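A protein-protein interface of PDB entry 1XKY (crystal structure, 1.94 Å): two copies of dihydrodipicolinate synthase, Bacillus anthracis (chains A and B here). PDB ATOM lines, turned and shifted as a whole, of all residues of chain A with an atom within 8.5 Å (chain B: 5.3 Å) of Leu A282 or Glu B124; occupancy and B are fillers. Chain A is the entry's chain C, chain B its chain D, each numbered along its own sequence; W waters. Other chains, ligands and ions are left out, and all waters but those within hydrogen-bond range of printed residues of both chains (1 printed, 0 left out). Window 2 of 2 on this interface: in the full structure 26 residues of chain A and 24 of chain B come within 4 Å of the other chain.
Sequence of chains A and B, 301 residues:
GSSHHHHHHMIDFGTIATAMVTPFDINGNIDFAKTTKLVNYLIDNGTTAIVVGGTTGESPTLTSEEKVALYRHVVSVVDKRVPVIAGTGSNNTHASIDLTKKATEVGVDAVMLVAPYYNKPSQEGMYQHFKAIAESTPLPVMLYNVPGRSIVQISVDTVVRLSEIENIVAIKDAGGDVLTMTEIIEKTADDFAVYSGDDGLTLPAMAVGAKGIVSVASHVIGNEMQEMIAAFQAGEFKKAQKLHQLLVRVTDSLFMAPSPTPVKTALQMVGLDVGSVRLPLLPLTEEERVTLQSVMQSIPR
Water W1 lies within hydrogen-bond range of the backbone carbonyl oxygen (O) of Pro A280 (2.9 Å) and the backbone NH (N) of Ser B122 (2.9 Å).
Ala A257 touches none of the printed residues of chain B.
Of the printed residues of chain B, Pro A280 touches Gly B125 (3.2 Å) and His B129 (3.8 Å).
Leu A282 touches three residues of chain B.
Of the printed residues of chain A, Ser B122 touches Pro A258 (3.7 Å).
Gly B125 touches just these residues of chain A: Pro A280 (3.2 Å) and Leu A282 (3.6 Å).
Tyr B127 touches none of the printed residues of chain A.
The nearest residue of chain A that does not touch Glu B124 is Pro A280 (5.7 Å).
No position is printed for both chains.
Of the 7 pairs that touch across the chains among the printed residues, none has its exchanged pair printed and touching as well.
Of the 9 printed residues of chain B, 5 touch a printed residue of chain A.
Printed residues of chain B that touch a printed residue of chain A: Ser B122, Glu B124, Gly B125, Gln B128 and His B129.
Of the 19 printed residues of chain A, 4 touch a printed residue of chain B.
Hydrophobic or aromatic side chains of chain A that line the printed part of chain B: Pro A258, Leu A279, Pro A280 and Leu A282.
Along chain A the printed residues that touch a printed residue of chain B span positions 258 to 282.
Among the printed residues, no Asp or Glu carboxylate lies within 4 Å of a Lys or Arg side-chain nitrogen of the other chain.
Among the printed residues, merely in contact across the chains: Pro A280 with Gly B125, Leu A282 with Glu B124, Leu A282 with Gly B125, Pro A258 with Ser B122, Pro A280 with His B129, Leu A282 with Gln B128 and Leu A279 with Gln B128.
O of Pro A258 is in hydrogen-bond range of OG1 of Thr A261 (3.3 Å).
OG1 of Thr A261 sits close to O of Leu A282 (3.5 Å).
OG of Ser B122 lies within hydrogen-bond range of N of Gly B125 (3.0 Å).
The side-chain amide oxygen (OE1) of Gln B128 sits close to the side-chain carboxylate (OE2) of Glu B124 (2.9 Å).
OE1 of Glu B124 lies within salt-bridge range of NH1 of Arg B161.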
ATOM      1  N   GLU A  58     -19.119   8.148 -19.614  1.00  0.00           N
ATOM      2  CA  GLU A  58     -18.786   9.208 -18.656  1.00  0.00           C
ATOM      3  C   GLU A  58     -19.570  10.504 -18.849  1.00  0.00           C
ATOM      4  O   GLU A  58     -19.027  11.609 -18.704  1.00  0.00           O
ATOM      5  CB  GLU A  58     -17.270   9.444 -18.615  1.00  0.00           C
ATOM      6  CG  GLU A  58     -16.534   8.294 -17.922  1.00  0.00           C
ATOM      7  CD  GLU A  58     -15.029   8.355 -18.124  1.00  0.00           C
ATOM      8  OE1 GLU A  58     -14.533   7.706 -19.066  1.00  0.00           O
ATOM      9  OE2 GLU A  58     -14.354   9.061 -17.342  1.00  0.00           O
ATOM     10  N   ALA A 257     -13.939  -2.331  -9.940  1.00  0.00           N
ATOM     11  CA  ALA A 257     -13.695  -0.905  -9.694  1.00  0.00           C
ATOM     12  C   ALA A 257     -14.815  -0.140 -10.401  1.00  0.00           C
ATOM     13  O   ALA A 257     -15.523  -0.719 -11.231  1.00  0.00           O
ATOM     14  CB  ALA A 257     -12.334  -0.492 -10.236  1.00  0.00           C
ATOM     15  N   PRO A 258     -15.009   1.144 -10.061  1.00  0.00           N
ATOM     16  CA  PRO A 258     -16.069   1.890 -10.758  1.00  0.00           C
ATOM     17  C   PRO A 258     -15.919   1.933 -12.286  1.00  0.00           C
ATOM     18  O   PRO A 258     -14.865   2.317 -12.823  1.00  0.00           O
ATOM     19  CB  PRO A 258     -15.980   3.289 -10.145  1.00  0.00           C
ATOM     20  CG  PRO A 258     -15.384   3.060  -8.790  1.00  0.00           C
ATOM     21  CD  PRO A 258     -14.378   1.960  -9.008  1.00  0.00           C
ATOM     22  N   SER A 259     -16.978   1.536 -12.984  1.00  0.00           N
ATOM     23  CA  SER A 259     -17.006   1.602 -14.440  1.00  0.00           C
ATOM     24  C   SER A 259     -17.070   3.046 -14.925  1.00  0.00           C
ATOM     25  O   SER A 259     -17.835   3.855 -14.399  1.00  0.00           O
ATOM     26  CB  SER A 259     -18.194   0.810 -14.990  1.00  0.00           C
ATOM     27  OG  SER A 259     -18.117   0.687 -16.398  1.00  0.00           O
ATOM     28  N   PRO A 260     -16.261   3.364 -15.931  1.00  0.00           N
ATOM     29  CA  PRO A 260     -15.926   2.399 -16.983  1.00  0.00           C
ATOM     30  C   PRO A 260     -14.447   2.029 -16.962  1.00  0.00           C
ATOM     31  O   PRO A 260     -13.908   1.584 -17.975  1.00  0.00           O
ATOM     32  CB  PRO A 260     -16.259   3.161 -18.267  1.00  0.00           C
ATOM     33  CG  PRO A 260     -16.061   4.591 -17.908  1.00  0.00           C
ATOM     34  CD  PRO A 260     -16.472   4.719 -16.468  1.00  0.00           C
ATOM     35  N   THR A 261     -13.803   2.213 -15.814  1.00  0.00           N
ATOM     36  CA  THR A 261     -12.347   2.259 -15.752  1.00  0.00           C
ATOM     37  C   THR A 261     -11.736   0.913 -16.125  1.00  0.00           C
ATOM     38  O   THR A 261     -10.751   0.849 -16.860  1.00  0.00           O
ATOM     39  CB  THR A 261     -11.879   2.681 -14.348  1.00  0.00           C
ATOM     40  OG1 THR A 261     -12.367   3.997 -14.054  1.00  0.00           O
ATOM     41  CG2 THR A 261     -10.368   2.856 -14.319  1.00  0.00           C
ATOM     42  N   PRO A 262     -12.328  -0.163 -15.614  1.00  0.00           N
ATOM     43  CA  PRO A 262     -11.894  -1.527 -15.972  1.00  0.00           C
ATOM     44  C   PRO A 262     -12.047  -1.880 -17.458  1.00  0.00           C
ATOM     45  O   PRO A 262     -11.112  -2.446 -18.046  1.00  0.00           O
ATOM     46  CB  PRO A 262     -12.772  -2.425 -15.083  1.00  0.00           C
ATOM     47  CG  PRO A 262     -13.181  -1.546 -13.948  1.00  0.00           C
ATOM     48  CD  PRO A 262     -13.366  -0.190 -14.570  1.00  0.00           C
ATOM     49  N   THR A 265      -9.404  -0.124 -19.405  1.00  0.00           N
ATOM     50  CA  THR A 265      -8.151  -0.822 -19.146  1.00  0.00           C
ATOM     51  C   THR A 265      -8.087  -2.147 -19.937  1.00  0.00           C
ATOM     52  O   THR A 265      -7.057  -2.475 -20.537  1.00  0.00           O
ATOM     53  CB  THR A 265      -7.971  -1.070 -17.620  1.00  0.00           C
ATOM     54  OG1 THR A 265      -8.230   0.151 -16.904  1.00  0.00           O
ATOM     55  CG2 THR A 265      -6.561  -1.535 -17.297  1.00  0.00           C
ATOM     56  N   SER A 276      -7.745   7.005 -20.367  1.00  0.00           N
ATOM     57  CA  SER A 276      -8.162   6.755 -18.996  1.00  0.00           C
ATOM     58  C   SER A 276      -9.475   7.502 -18.719  1.00  0.00           C
ATOM     59  O   SER A 276     -10.280   7.702 -19.638  1.00  0.00           O
ATOM     60  CB  SER A 276      -7.033   7.153 -18.037  1.00  0.00           C
ATOM     61  OG  SER A 276      -7.305   6.735 -16.712  1.00  0.00           O
ATOM     62  N   VAL A 277      -9.689   7.905 -17.469  1.00  0.00           N
ATOM     63  CA  VAL A 277     -10.987   8.433 -17.023  1.00  0.00           C
ATOM     64  C   VAL A 277     -10.852   9.804 -16.385  1.00  0.00           C
ATOM     65  O   VAL A 277      -9.760  10.206 -16.009  1.00  0.00           O
ATOM     66  CB  VAL A 277     -11.676   7.472 -16.014  1.00  0.00           C
ATOM     67  CG1 VAL A 277     -12.139   6.183 -16.722  1.00  0.00           C
ATOM     68  CG2 VAL A 277     -10.761   7.145 -14.831  1.00  0.00           C
ATOM     69  N   ARG A 278     -11.976  10.504 -16.246  1.00  0.00           N
ATOM     70  CA  ARG A 278     -12.012  11.810 -15.582  1.00  0.00           C
ATOM     71  C   ARG A 278     -12.445  11.678 -14.126  1.00  0.00           C
ATOM     72  O   ARG A 278     -13.287  10.839 -13.773  1.00  0.00           O
ATOM     73  CB  ARG A 278     -12.957  12.767 -16.320  1.00  0.00           C
ATOM     74  CG  ARG A 278     -12.515  13.100 -17.728  1.00  0.00           C
ATOM     75  CD  ARG A 278     -13.501  14.021 -18.425  1.00  0.00           C
ATOM     76  NE  ARG A 278     -13.044  14.415 -19.755  1.00  0.00           N
ATOM     77  CZ  ARG A 278     -13.697  15.258 -20.562  1.00  0.00           C
ATOM     78  NH1 ARG A 278     -14.852  15.804 -20.190  1.00  0.00           N
ATOM     79  NH2 ARG A 278     -13.195  15.555 -21.751  1.00  0.00           N
ATOM     80  N   LEU A 279     -11.853  12.509 -13.282  1.00  0.00           N
ATOM     81  CA  LEU A 279     -12.264  12.618 -11.895  1.00  0.00           C
ATOM     82  C   LEU A 279     -13.771  12.926 -11.819  1.00  0.00           C
ATOM     83  O   LEU A 279     -14.278  13.738 -12.605  1.00  0.00           O
ATOM     84  CB  LEU A 279     -11.442  13.700 -11.189  1.00  0.00           C
ATOM     85  CG  LEU A 279     -10.010  13.310 -10.788  1.00  0.00           C
ATOM     86  CD1 LEU A 279      -9.218  14.563 -10.500  1.00  0.00           C
ATOM     87  CD2 LEU A 279     -10.008  12.399  -9.578  1.00  0.00           C
ATOM     88  N   PRO A 280     -14.476  12.330 -10.846  1.00  0.00           N
ATOM     89  CA  PRO A 280     -13.977  11.614  -9.662  1.00  0.00           C
ATOM     90  C   PRO A 280     -13.547  10.143  -9.851  1.00  0.00           C
ATOM     91  O   PRO A 280     -13.251   9.465  -8.865  1.00  0.00           O
ATOM     92  CB  PRO A 280     -15.159  11.710  -8.699  1.00  0.00           C
ATOM     93  CG  PRO A 280     -16.355  11.634  -9.610  1.00  0.00           C
ATOM     94  CD  PRO A 280     -15.951  12.380 -10.867  1.00  0.00           C
ATOM     95  N   LEU A 281     -13.497   9.663 -11.091  1.00  0.00           N
ATOM     96  CA  LEU A 281     -12.983   8.318 -11.373  1.00  0.00           C
ATOM     97  C   LEU A 281     -11.457   8.331 -11.510  1.00  0.00           C
ATOM     98  O   LEU A 281     -10.867   9.341 -11.894  1.00  0.00           O
ATOM     99  CB  LEU A 281     -13.623   7.741 -12.642  1.00  0.00           C
ATOM    100  CG  LEU A 281     -15.150   7.709 -12.666  1.00  0.00           C
ATOM    101  CD1 LEU A 281     -15.639   6.991 -13.900  1.00  0.00           C
ATOM    102  CD2 LEU A 281     -15.729   7.062 -11.412  1.00  0.00           C
ATOM    103  N   LEU A 282     -10.838   7.197 -11.190  1.00  0.00           N
ATOM    104  CA  LEU A 282      -9.378   7.061 -11.172  1.00  0.00           C
ATOM    105  C   LEU A 282      -8.921   5.831 -11.953  1.00  0.00           C
ATOM    106  O   LEU A 282      -9.658   4.854 -12.053  1.00  0.00           O
ATOM    107  CB  LEU A 282      -8.892   6.938  -9.728  1.00  0.00           C
ATOM    108  CG  LEU A 282      -8.998   8.169  -8.834  1.00  0.00           C
ATOM    109  CD1 LEU A 282      -8.559   7.799  -7.433  1.00  0.00           C
ATOM    110  CD2 LEU A 282      -8.162   9.321  -9.359  1.00  0.00           C
ATOM    111  N   PRO A 283      -7.690   5.866 -12.496  1.00  0.00           N
ATOM    112  CA  PRO A 283      -7.096   4.632 -13.040  1.00  0.00           C
ATOM    113  C   PRO A 283      -7.027   3.504 -12.009  1.00  0.00           C
ATOM    114  O   PRO A 283      -6.933   3.760 -10.805  1.00  0.00           O
ATOM    115  CB  PRO A 283      -5.676   5.055 -13.428  1.00  0.00           C
ATOM    116  CG  PRO A 283      -5.722   6.544 -13.561  1.00  0.00           C
ATOM    117  CD  PRO A 283      -6.786   7.023 -12.621  1.00  0.00           C
ATOM    118  N   LEU A 284      -7.087   2.265 -12.496  1.00  0.00           N
ATOM    119  CA  LEU A 284      -6.897   1.087 -11.659  1.00  0.00           C
ATOM    120  C   LEU A 284      -5.530   1.138 -10.993  1.00  0.00           C
ATOM    121  O   LEU A 284      -4.570   1.644 -11.573  1.00  0.00           O
ATOM    122  CB  LEU A 284      -7.002  -0.206 -12.490  1.00  0.00           C
ATOM    123  CG  LEU A 284      -8.376  -0.863 -12.685  1.00  0.00           C
ATOM    124  CD1 LEU A 284      -9.456   0.089 -13.023  1.00  0.00           C
ATOM    125  CD2 LEU A 284      -8.276  -1.932 -13.749  1.00  0.00           C
ATOM    126  N   THR A 285      -5.472   0.635  -9.767  1.00  0.00           N
ATOM    127  CA  THR A 285      -4.209   0.346  -9.106  1.00  0.00           C
ATOM    128  C   THR A 285      -3.579  -0.869  -9.783  1.00  0.00           C
ATOM    129  O   THR A 285      -4.245  -1.614 -10.518  1.00  0.00           O
ATOM    130  CB  THR A 285      -4.395   0.030  -7.612  1.00  0.00           C
ATOM    131  OG1 THR A 285      -5.146  -1.180  -7.447  1.00  0.00           O
ATOM    132  CG2 THR A 285      -5.118   1.181  -6.889  1.00  0.00           C
ATOM    133  N   GLU A 288      -5.513  -3.935  -8.824  1.00  0.00           N
ATOM    134  CA  GLU A 288      -6.743  -4.042  -9.606  1.00  0.00           C
ATOM    135  C   GLU A 288      -6.462  -4.494 -11.043  1.00  0.00           C
ATOM    136  O   GLU A 288      -7.189  -5.325 -11.580  1.00  0.00           O
ATOM    137  CB  GLU A 288      -7.505  -2.705  -9.602  1.00  0.00           C
ATOM    138  CG  GLU A 288      -8.092  -2.343  -8.242  1.00  0.00           C
ATOM    139  CD  GLU A 288      -8.639  -0.919  -8.153  1.00  0.00           C
ATOM    140  OE1 GLU A 288      -8.077   0.007  -8.777  1.00  0.00           O
ATOM    141  OE2 GLU A 288      -9.638  -0.722  -7.430  1.00  0.00           O
ATOM    142  N   SER B 122     -15.247   5.451  -6.002  1.00  0.00           N
ATOM    143  CA  SER B 122     -14.654   4.720  -4.909  1.00  0.00           C
ATOM    144  C   SER B 122     -14.271   5.685  -3.786  1.00  0.00           C
ATOM    145  O   SER B 122     -14.341   6.906  -3.943  1.00  0.00           O
ATOM    146  CB  SER B 122     -13.386   4.023  -5.410  1.00  0.00           C
ATOM    147  OG  SER B 122     -12.416   5.002  -5.759  1.00  0.00           O
ATOM    148  N   GLN B 123     -13.818   5.117  -2.670  1.00  0.00           N
ATOM    149  CA  GLN B 123     -13.342   5.915  -1.541  1.00  0.00           C
ATOM    150  C   GLN B 123     -12.181   6.815  -1.943  1.00  0.00           C
ATOM    151  O   GLN B 123     -12.180   8.005  -1.629  1.00  0.00           O
ATOM    152  CB  GLN B 123     -12.945   5.007  -0.374  1.00  0.00           C
ATOM    153  CG  GLN B 123     -14.124   4.263   0.222  1.00  0.00           C
ATOM    154  CD  GLN B 123     -15.242   5.200   0.667  1.00  0.00           C
ATOM    155  OE1 GLN B 123     -15.002   6.166   1.390  1.00  0.00           O
ATOM    156  NE2 GLN B 123     -16.466   4.919   0.231  1.00  0.00           N
ATOM    157  N   GLU B 124     -11.216   6.259  -2.671  1.00  0.00           N
ATOM    158  CA  GLU B 124     -10.041   7.038  -3.105  1.00  0.00           C
ATOM    159  C   GLU B 124     -10.410   8.059  -4.179  1.00  0.00           C
ATOM    160  O   GLU B 124      -9.854   9.154  -4.205  1.00  0.00           O
ATOM    161  CB  GLU B 124      -8.907   6.113  -3.589  1.00  0.00           C
ATOM    162  CG  GLU B 124      -7.625   6.836  -4.044  1.00  0.00           C
ATOM    163  CD  GLU B 124      -6.926   7.620  -2.936  1.00  0.00           C
ATOM    164  OE1 GLU B 124      -7.200   7.377  -1.743  1.00  0.00           O
ATOM    165  OE2 GLU B 124      -6.088   8.480  -3.261  1.00  0.00           O
ATOM    166  N   GLY B 125     -11.330   7.700  -5.067  1.00  0.00           N
ATOM    167  CA  GLY B 125     -11.871   8.654  -6.040  1.00  0.00           C
ATOM    168  C   GLY B 125     -12.494   9.856  -5.351  1.00  0.00           C
ATOM    169  O   GLY B 125     -12.240  10.998  -5.719  1.00  0.00           O
ATOM    170  N   MET B 126     -13.302   9.598  -4.331  1.00  0.00           N
ATOM    171  CA  MET B 126     -13.938  10.673  -3.567  1.00  0.00           C
ATOM    172  C   MET B 126     -12.898  11.489  -2.821  1.00  0.00           C
ATOM    173  O   MET B 126     -12.987  12.712  -2.756  1.00  0.00           O
ATOM    174  CB  MET B 126     -14.976  10.099  -2.609  1.00  0.00           C
ATOM    175  CG  MET B 126     -16.239   9.688  -3.317  1.00  0.00           C
ATOM    176  SD  MET B 126     -17.591   9.340  -2.199  1.00  0.00           S
ATOM    177  CE  MET B 126     -17.172   7.683  -1.683  1.00  0.00           C
ATOM    178  N   TYR B 127     -11.882  10.817  -2.289  1.00  0.00           N
ATOM    179  CA  TYR B 127     -10.806  11.517  -1.604  1.00  0.00           C
ATOM    180  C   TYR B 127     -10.122  12.508  -2.547  1.00  0.00           C
ATOM    181  O   TYR B 127      -9.939  13.680  -2.201  1.00  0.00           O
ATOM    182  CB  TYR B 127      -9.783  10.540  -1.028  1.00  0.00           C
ATOM    183  CG  TYR B 127      -8.626  11.256  -0.406  1.00  0.00           C
ATOM    184  CD1 TYR B 127      -8.727  11.796   0.877  1.00  0.00           C
ATOM    185  CD2 TYR B 127      -7.435  11.433  -1.110  1.00  0.00           C
ATOM    186  CE1 TYR B 127      -7.663  12.476   1.452  1.00  0.00           C
ATOM    187  CE2 TYR B 127      -6.372  12.115  -0.546  1.00  0.00           C
ATOM    188  CZ  TYR B 127      -6.486  12.630   0.730  1.00  0.00           C
ATOM    189  OH  TYR B 127      -5.426  13.306   1.288  1.00  0.00           O
ATOM    190  N   GLN B 128      -9.770  12.042  -3.741  1.00  0.00           N
ATOM    191  CA  GLN B 128      -9.101  12.888  -4.729  1.00  0.00           C
ATOM    192  C   GLN B 128     -10.043  13.981  -5.245  1.00  0.00           C
ATOM    193  O   GLN B 128      -9.596  15.099  -5.507  1.00  0.00           O
ATOM    194  CB  GLN B 128      -8.543  12.050  -5.886  1.00  0.00           C
ATOM    195  CG  GLN B 128      -7.413  11.077  -5.501  1.00  0.00           C
ATOM    196  CD  GLN B 128      -6.196  11.771  -4.890  1.00  0.00           C
ATOM    197  OE1 GLN B 128      -5.509  11.213  -4.030  1.00  0.00           O
ATOM    198  NE2 GLN B 128      -5.937  12.990  -5.323  1.00  0.00           N
ATOM    199  N   HIS B 129     -11.331  13.643  -5.376  1.00  0.00           N
ATOM    200  CA  HIS B 129     -12.395  14.589  -5.757  1.00  0.00           C
ATOM    201  C   HIS B 129     -12.453  15.742  -4.761  1.00  0.00           C
ATOM    202  O   HIS B 129     -12.266  16.903  -5.119  1.00  0.00           O
ATOM    203  CB  HIS B 129     -13.751  13.855  -5.835  1.00  0.00           C
ATOM    204  CG  HIS B 129     -14.942  14.751  -6.035  1.00  0.00           C
ATOM    205  ND1 HIS B 129     -15.309  15.244  -7.270  1.00  0.00           N
ATOM    206  CD2 HIS B 129     -15.876  15.204  -5.160  1.00  0.00           C
ATOM    207  CE1 HIS B 129     -16.396  15.988  -7.143  1.00  0.00           C
ATOM    208  NE2 HIS B 129     -16.763  15.977  -5.871  1.00  0.00           N
ATOM    209  N   ARG B 161      -9.308  11.184   6.842  1.00  0.00           N
ATOM    210  CA  ARG B 161      -8.229  11.653   5.963  1.00  0.00           C
ATOM    211  C   ARG B 161      -8.499  13.058   5.425  1.00  0.00           C
ATOM    212  O   ARG B 161      -7.594  13.891   5.353  1.00  0.00           O
ATOM    213  CB  ARG B 161      -8.053  10.707   4.771  1.00  0.00           C
ATOM    214  CG  ARG B 161      -7.509   9.330   5.135  1.00  0.00           C
ATOM    215  CD  ARG B 161      -7.617   8.414   3.936  1.00  0.00           C
ATOM    216  NE  ARG B 161      -6.688   8.823   2.889  1.00  0.00           N
ATOM    217  CZ  ARG B 161      -6.826   8.557   1.590  1.00  0.00           C
ATOM    218  NH1 ARG B 161      -7.878   7.890   1.128  1.00  0.00           N
ATOM    219  NH2 ARG B 161      -5.902   8.973   0.743  1.00  0.00           N
HETATM  220  O   HOH W   1     -13.942   6.751  -8.257  1.00  0.00           O
